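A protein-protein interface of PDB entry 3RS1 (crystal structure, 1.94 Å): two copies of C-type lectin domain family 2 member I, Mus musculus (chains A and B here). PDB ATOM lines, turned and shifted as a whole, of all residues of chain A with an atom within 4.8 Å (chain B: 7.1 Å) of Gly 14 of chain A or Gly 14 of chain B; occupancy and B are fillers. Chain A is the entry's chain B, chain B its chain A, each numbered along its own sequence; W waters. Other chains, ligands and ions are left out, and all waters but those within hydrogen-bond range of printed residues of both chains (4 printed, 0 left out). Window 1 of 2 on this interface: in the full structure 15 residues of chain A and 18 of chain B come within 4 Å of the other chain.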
ATOM      1  N   CYS A   8     -10.795 -18.534 -24.925  1.00  0.00           N
ATOM      2  CA  CYS A   8     -10.850 -17.429 -25.881  1.00  0.00           C
ATOM      3  C   CYS A   8     -11.944 -16.456 -25.414  1.00  0.00           C
ATOM      4  O   CYS A   8     -12.889 -16.843 -24.701  1.00  0.00           O
ATOM      5  CB  CYS A   8     -11.089 -17.961 -27.288  1.00  0.00           C
ATOM      6  SG  CYS A   8      -9.688 -18.967 -27.930  1.00  0.00           S
ATOM      7  N   TRP A  12     -14.840 -15.725 -29.952  1.00  0.00           N
ATOM      8  CA  TRP A  12     -13.612 -16.199 -30.589  1.00  0.00           C
ATOM      9  C   TRP A  12     -13.513 -17.708 -30.442  1.00  0.00           C
ATOM     10  O   TRP A  12     -14.070 -18.282 -29.515  1.00  0.00           O
ATOM     11  CB  TRP A  12     -12.386 -15.540 -29.948  1.00  0.00           C
ATOM     12  CG  TRP A  12     -12.290 -14.040 -30.155  1.00  0.00           C
ATOM     13  CD1 TRP A  12     -13.158 -13.081 -29.688  1.00  0.00           C
ATOM     14  CD2 TRP A  12     -11.230 -13.330 -30.820  1.00  0.00           C
ATOM     15  NE1 TRP A  12     -12.699 -11.820 -30.033  1.00  0.00           N
ATOM     16  CE2 TRP A  12     -11.539 -11.947 -30.749  1.00  0.00           C
ATOM     17  CE3 TRP A  12     -10.066 -13.729 -31.497  1.00  0.00           C
ATOM     18  CZ2 TRP A  12     -10.717 -10.956 -31.323  1.00  0.00           C
ATOM     19  CZ3 TRP A  12      -9.250 -12.740 -32.068  1.00  0.00           C
ATOM     20  CH2 TRP A  12      -9.597 -11.368 -31.980  1.00  0.00           C
ATOM     21  N   THR A  13     -12.822 -18.350 -31.375  1.00  0.00           N
ATOM     22  CA  THR A  13     -12.730 -19.789 -31.405  1.00  0.00           C
ATOM     23  C   THR A  13     -11.269 -20.172 -31.339  1.00  0.00           C
ATOM     24  O   THR A  13     -10.446 -19.535 -31.958  1.00  0.00           O
ATOM     25  CB  THR A  13     -13.337 -20.377 -32.688  1.00  0.00           C
ATOM     26  OG1 THR A  13     -14.716 -20.019 -32.767  1.00  0.00           O
ATOM     27  CG2 THR A  13     -13.239 -21.884 -32.657  1.00  0.00           C
ATOM     28  N   GLY A  14     -10.973 -21.210 -30.562  1.00  0.00           N
ATOM     29  CA  GLY A  14      -9.618 -21.655 -30.324  1.00  0.00           C
ATOM     30  C   GLY A  14      -9.188 -22.851 -31.144  1.00  0.00           C
ATOM     31  O   GLY A  14      -9.924 -23.814 -31.297  1.00  0.00           O
ATOM     32  N   VAL A  15      -7.989 -22.762 -31.713  1.00  0.00           N
ATOM     33  CA  VAL A  15      -7.267 -23.936 -32.187  1.00  0.00           C
ATOM     34  C   VAL A  15      -5.906 -23.857 -31.537  1.00  0.00           C
ATOM     35  O   VAL A  15      -5.146 -22.909 -31.792  1.00  0.00           O
ATOM     36  CB  VAL A  15      -7.118 -23.947 -33.707  1.00  0.00           C
ATOM     37  CG1 VAL A  15      -6.358 -25.205 -34.164  1.00  0.00           C
ATOM     38  CG2 VAL A  15      -8.495 -23.840 -34.388  1.00  0.00           C
ATOM     39  N   GLY A  16      -5.599 -24.823 -30.664  1.00  0.00           N
ATOM     40  CA  GLY A  16      -4.331 -24.815 -29.961  1.00  0.00           C
ATOM     41  C   GLY A  16      -4.229 -23.610 -29.047  1.00  0.00           C
ATOM     42  O   GLY A  16      -5.199 -23.297 -28.335  1.00  0.00           O
ATOM     43  N   LYS A  18      -4.075 -20.559 -30.177  1.00  0.00           N
ATOM     44  CA  LYS A  18      -4.556 -19.406 -30.933  1.00  0.00           C
ATOM     45  C   LYS A  18      -6.029 -19.159 -30.637  1.00  0.00           C
ATOM     46  O   LYS A  18      -6.779 -20.094 -30.324  1.00  0.00           O
ATOM     47  CB  LYS A  18      -4.388 -19.630 -32.424  1.00  0.00           C
ATOM     48  CG  LYS A  18      -2.941 -19.733 -32.956  1.00  0.00           C
ATOM     49  CD  LYS A  18      -2.364 -18.424 -33.495  1.00  0.00           C
ATOM     50  CE  LYS A  18      -1.583 -18.625 -34.805  1.00  0.00           C
ATOM     51  NZ  LYS A  18      -0.450 -19.614 -34.664  1.00  0.00           N
ATOM     52  N   CYS A  19      -6.449 -17.902 -30.743  1.00  0.00           N
ATOM     53  CA  CYS A  19      -7.874 -17.565 -30.797  1.00  0.00           C
ATOM     54  C   CYS A  19      -8.205 -16.799 -32.111  1.00  0.00           C
ATOM     55  O   CYS A  19      -7.451 -15.889 -32.514  1.00  0.00           O
ATOM     56  CB  CYS A  19      -8.277 -16.749 -29.578  1.00  0.00           C
ATOM     57  SG  CYS A  19      -8.146 -17.595 -27.987  1.00  0.00           S
ATOM     58  N   LYS B   3     -10.563 -22.821 -18.539  1.00  0.00           N
ATOM     59  CA  LYS B   3     -10.314 -24.170 -19.026  1.00  0.00           C
ATOM     60  C   LYS B   3      -9.420 -24.933 -18.024  1.00  0.00           C
ATOM     61  O   LYS B   3      -8.548 -24.354 -17.411  1.00  0.00           O
ATOM     62  CB  LYS B   3      -9.602 -24.097 -20.376  1.00  0.00           C
ATOM     63  CG  LYS B   3     -10.239 -23.142 -21.396  1.00  0.00           C
ATOM     64  CD  LYS B   3      -9.611 -23.249 -22.777  1.00  0.00           C
ATOM     65  CE  LYS B   3      -8.128 -22.929 -22.757  1.00  0.00           C
ATOM     66  NZ  LYS B   3      -7.543 -22.880 -24.103  1.00  0.00           N
ATOM     67  N   CYS B   8      -7.275 -27.554 -26.202  1.00  0.00           N
ATOM     68  CA  CYS B   8      -7.928 -28.772 -26.633  1.00  0.00           C
ATOM     69  C   CYS B   8      -6.839 -29.705 -27.131  1.00  0.00           C
ATOM     70  O   CYS B   8      -5.766 -29.256 -27.529  1.00  0.00           O
ATOM     71  CB  CYS B   8      -8.924 -28.494 -27.774  1.00  0.00           C
ATOM     72  SG  CYS B   8     -10.461 -27.564 -27.317  1.00  0.00           S
ATOM     73  N   TRP B  12      -8.993 -30.972 -32.217  1.00  0.00           N
ATOM     74  CA  TRP B  12     -10.239 -30.470 -31.666  1.00  0.00           C
ATOM     75  C   TRP B  12     -10.191 -28.945 -31.554  1.00  0.00           C
ATOM     76  O   TRP B  12      -9.121 -28.350 -31.459  1.00  0.00           O
ATOM     77  CB  TRP B  12     -10.492 -31.105 -30.289  1.00  0.00           C
ATOM     78  CG  TRP B  12     -10.655 -32.602 -30.342  1.00  0.00           C
ATOM     79  CD1 TRP B  12      -9.743 -33.521 -30.801  1.00  0.00           C
ATOM     80  CD2 TRP B  12     -11.794 -33.347 -29.911  1.00  0.00           C
ATOM     81  NE1 TRP B  12     -10.253 -34.794 -30.683  1.00  0.00           N
ATOM     82  CE2 TRP B  12     -11.510 -34.715 -30.132  1.00  0.00           C
ATOM     83  CE3 TRP B  12     -13.020 -32.994 -29.339  1.00  0.00           C
ATOM     84  CZ2 TRP B  12     -12.427 -35.734 -29.823  1.00  0.00           C
ATOM     85  CZ3 TRP B  12     -13.922 -34.023 -29.002  1.00  0.00           C
ATOM     86  CH2 TRP B  12     -13.620 -35.359 -29.270  1.00  0.00           C
ATOM     87  N   THR B  13     -11.370 -28.338 -31.552  1.00  0.00           N
ATOM     88  CA  THR B  13     -11.555 -26.904 -31.634  1.00  0.00           C
ATOM     89  C   THR B  13     -12.407 -26.428 -30.442  1.00  0.00           C
ATOM     90  O   THR B  13     -13.387 -27.080 -30.040  1.00  0.00           O
ATOM     91  CB  THR B  13     -12.254 -26.525 -32.938  1.00  0.00           C
ATOM     92  OG1 THR B  13     -11.498 -27.005 -34.067  1.00  0.00           O
ATOM     93  CG2 THR B  13     -12.453 -25.040 -33.023  1.00  0.00           C
ATOM     94  N   GLY B  14     -12.029 -25.278 -29.897  1.00  0.00           N
ATOM     95  CA  GLY B  14     -12.516 -24.857 -28.600  1.00  0.00           C
ATOM     96  C   GLY B  14     -13.394 -23.642 -28.713  1.00  0.00           C
ATOM     97  O   GLY B  14     -13.106 -22.742 -29.513  1.00  0.00           O
ATOM     98  N   VAL B  15     -14.507 -23.681 -27.973  1.00  0.00           N
ATOM     99  CA  VAL B  15     -15.413 -22.541 -27.753  1.00  0.00           C
ATOM    100  C   VAL B  15     -15.556 -22.512 -26.236  1.00  0.00           C
ATOM    101  O   VAL B  15     -15.976 -23.509 -25.622  1.00  0.00           O
ATOM    102  CB  VAL B  15     -16.832 -22.715 -28.370  1.00  0.00           C
ATOM    103  CG1 VAL B  15     -17.722 -21.552 -27.988  1.00  0.00           C
ATOM    104  CG2 VAL B  15     -16.786 -22.800 -29.897  1.00  0.00           C
ATOM    105  N   GLY B  16     -15.203 -21.390 -25.624  1.00  0.00           N
ATOM    106  CA  GLY B  16     -15.112 -21.320 -24.167  1.00  0.00           C
ATOM    107  C   GLY B  16     -14.360 -22.534 -23.639  1.00  0.00           C
ATOM    108  O   GLY B  16     -13.273 -22.856 -24.127  1.00  0.00           O
ATOM    109  N   ASN B  17     -14.955 -23.227 -22.669  1.00  0.00           N
ATOM    110  CA  ASN B  17     -14.316 -24.387 -22.048  1.00  0.00           C
ATOM    111  C   ASN B  17     -14.744 -25.735 -22.637  1.00  0.00           C
ATOM    112  O   ASN B  17     -14.635 -26.760 -21.954  1.00  0.00           O
ATOM    113  CB  ASN B  17     -14.590 -24.410 -20.520  1.00  0.00           C
ATOM    114  CG  ASN B  17     -16.019 -24.842 -20.179  1.00  0.00           C
ATOM    115  OD1 ASN B  17     -16.950 -24.631 -20.952  1.00  0.00           O
ATOM    116  ND2 ASN B  17     -16.187 -25.457 -19.024  1.00  0.00           N
ATOM    117  N   LYS B  18     -15.255 -25.729 -23.861  1.00  0.00           N
ATOM    118  CA  LYS B  18     -15.616 -26.963 -24.591  1.00  0.00           C
ATOM    119  C   LYS B  18     -14.704 -27.151 -25.792  1.00  0.00           C
ATOM    120  O   LYS B  18     -14.146 -26.194 -26.307  1.00  0.00           O
ATOM    121  CB  LYS B  18     -17.048 -26.910 -25.097  1.00  0.00           C
ATOM    122  CG  LYS B  18     -18.113 -26.571 -24.049  1.00  0.00           C
ATOM    123  CD  LYS B  18     -18.737 -27.791 -23.406  1.00  0.00           C
ATOM    124  CE  LYS B  18     -20.235 -27.869 -23.685  1.00  0.00           C
ATOM    125  NZ  LYS B  18     -20.970 -26.710 -23.067  1.00  0.00           N
ATOM    126  N   CYS B  19     -14.566 -28.405 -26.208  1.00  0.00           N
ATOM    127  CA  CYS B  19     -13.701 -28.830 -27.287  1.00  0.00           C
ATOM    128  C   CYS B  19     -14.549 -29.692 -28.219  1.00  0.00           C
ATOM    129  O   CYS B  19     -15.282 -30.547 -27.757  1.00  0.00           O
ATOM    130  CB  CYS B  19     -12.552 -29.661 -26.742  1.00  0.00           C
ATOM    131  SG  CYS B  19     -11.296 -28.743 -25.836  1.00  0.00           S
ATOM    132  N   PHE B  20     -14.434 -29.471 -29.522  1.00  0.00           N
ATOM    133  CA  PHE B  20     -15.295 -30.092 -30.505  1.00  0.00           C
ATOM    134  C   PHE B  20     -14.500 -30.776 -31.610  1.00  0.00           C
ATOM    135  O   PHE B  20     -13.398 -30.351 -31.935  1.00  0.00           O
ATOM    136  CB  PHE B  20     -16.202 -29.038 -31.154  1.00  0.00           C
ATOM    137  CG  PHE B  20     -17.183 -28.413 -30.214  1.00  0.00           C
ATOM    138  CD1 PHE B  20     -16.920 -27.176 -29.624  1.00  0.00           C
ATOM    139  CD2 PHE B  20     -18.382 -29.033 -29.928  1.00  0.00           C
ATOM    140  CE1 PHE B  20     -17.846 -26.589 -28.793  1.00  0.00           C
ATOM    141  CE2 PHE B  20     -19.289 -28.458 -29.060  1.00  0.00           C
ATOM    142  CZ  PHE B  20     -19.031 -27.229 -28.506  1.00  0.00           C
ATOM    143  N   PHE B  54     -21.668 -21.737 -33.112  1.00  0.00           N
ATOM    144  CA  PHE B  54     -20.448 -22.408 -33.537  1.00  0.00           C
ATOM    145  C   PHE B  54     -20.758 -23.749 -34.211  1.00  0.00           C
ATOM    146  O   PHE B  54     -20.243 -24.013 -35.303  1.00  0.00           O
ATOM    147  CB  PHE B  54     -19.449 -22.566 -32.388  1.00  0.00           C
ATOM    148  CG  PHE B  54     -18.336 -23.532 -32.689  1.00  0.00           C
ATOM    149  CD1 PHE B  54     -17.219 -23.127 -33.358  1.00  0.00           C
ATOM    150  CD2 PHE B  54     -18.438 -24.853 -32.302  1.00  0.00           C
ATOM    151  CE1 PHE B  54     -16.202 -24.025 -33.664  1.00  0.00           C
ATOM    152  CE2 PHE B  54     -17.421 -25.759 -32.602  1.00  0.00           C
ATOM    153  CZ  PHE B  54     -16.313 -25.337 -33.273  1.00  0.00           C
ATOM    154  N   ASN B 122     -13.096 -29.010 -21.758  1.00  0.00           N
ATOM    155  CA  ASN B 122     -11.752 -28.728 -21.324  1.00  0.00           C
ATOM    156  C   ASN B 122     -11.752 -28.345 -19.833  1.00  0.00           C
ATOM    157  O   ASN B 122     -11.960 -27.173 -19.423  1.00  0.00           O
ATOM    158  CB  ASN B 122     -11.157 -27.618 -22.155  1.00  0.00           C
ATOM    159  CG  ASN B 122      -9.714 -27.422 -21.864  1.00  0.00           C
ATOM    160  OD1 ASN B 122      -9.252 -27.744 -20.764  1.00  0.00           O
ATOM    161  ND2 ASN B 122      -8.977 -26.891 -22.838  1.00  0.00           N
ATOM    162  OXT ASN B 122     -11.528 -29.218 -18.981  1.00  0.00           O
HETATM  163  O   HOH W   1     -15.036 -18.739 -27.255  1.00  0.00           O
HETATM  164  O   HOH W   2      -7.529 -25.041 -27.879  1.00  0.00           O
HETATM  165  O   HOH W   3      -6.543 -27.526 -31.308  1.00  0.00           O
HETATM  166  O   HOH W   4     -11.711 -21.157 -25.555  1.00  0.00           O
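The backbone carbonyl oxygen (O) of Gly 14 of chain B is in hydrogen-bond range of the backbone NH (N) of Gly 14 of chain A (2.8 Å).
The side-chain sulfur (SG) of Cys 8 of chain A is disulfide-bonded to the side-chain sulfur (SG) of Cys 19 of chain A (2.1 Å).
The backbone NH (N) of Gly 14 of chain A sits close to the side-chain sulfur (SG) of Cys 8 of chain A (3.7 Å).
N of Phe 20 of chain B is in hydrogen-bond range of O of Thr 13 of chain B (2.7 Å).
The backbone NH (N) of Gly 14 of chain B lies close to the side-chain sulfur (SG) of Cys 8 of chain B, 3.8 Å away.
SG of Cys 8 of chain B is disulfide-bonded to SG of Cys 19 of chain B, 2.1 Å away.
Thr 13 of chain A touches Thr 13 of chain B (CG2 to CG2, 3.3 Å).
Thr 13 of chain A touches Gly 14 of chain B (CG2 to O, 3.3 Å).
Thr 13 of chain A touches Phe 54 of chain B (CG2 to CE1, 3.8 Å).
Thr 13 of chain B touches Gly 14 of chain A.
Printed residues of chain B within 4 Å of Thr 13 of chain A: Thr 13, Gly 14 and Phe 54.
Printed residues of chain B within 4 Å of Gly 14 of chain A: Thr 13 and Gly 14.
Printed residues of chain A within 4 Å of Thr 13 of chain B: Thr 13 (3.3 Å) and Gly 14 (3.3 Å).
Of chain A, only Thr 13 and Gly 14 come within 4 Å of Gly 14 of chain B.
Phe 20 of chain B touches none of the printed residues of chain A.
Of the printed residues of chain A, Phe 54 of chain B touches Thr 13 (3.8 Å).
The nearest residue of chain B that does not touch Gly 14 of chain A is Trp 12 of chain B (4.6 Å).
The nearest residue of chain A that does not touch Gly 14 of chain B is Trp 12 of chain A (4.6 Å).
Hydrophobic or aromatic side chains of chain B within 4 Å of the printed part of chain A: Phe 54.
Among the printed residues, no Asp or Glu carboxylate lies within 4 Å of a Lys or Arg side-chain nitrogen of the other chain.
Thr 13 of chain B touches its own counterpart, Thr 13 of chain A.
Thr 13 of chain A touches Gly 14 of chain B, and with the chains exchanged Gly 14 of chain A touches Thr 13 of chain B.
Gly 14 of chain B touches its own counterpart, Gly 14 of chain A.
Of the 5 pairs that touch across the chains among the printed residues, 4 have their exchanged pair printed and touching as well.
Water W1 bridges O of Trp 12 of chain A (2.5 Å) and N of Gly 16 of chain B (3.1 Å).
Water W3 bridges the backbone carbonyl oxygen of Trp 12 of chain B (2.7 Å) and the backbone NH of Gly 16 of chain A (2.9 Å).
Water W4 bridges the backbone carbonyl oxygen of Gly 16 of chain B (2.7 Å) and the backbone NH of Cys 8 of chain A (2.8 Å).
Water W2 bridges O of Gly 16 of chain A (2.9 Å) and N of Cys 8 of chain B (3.0 Å).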
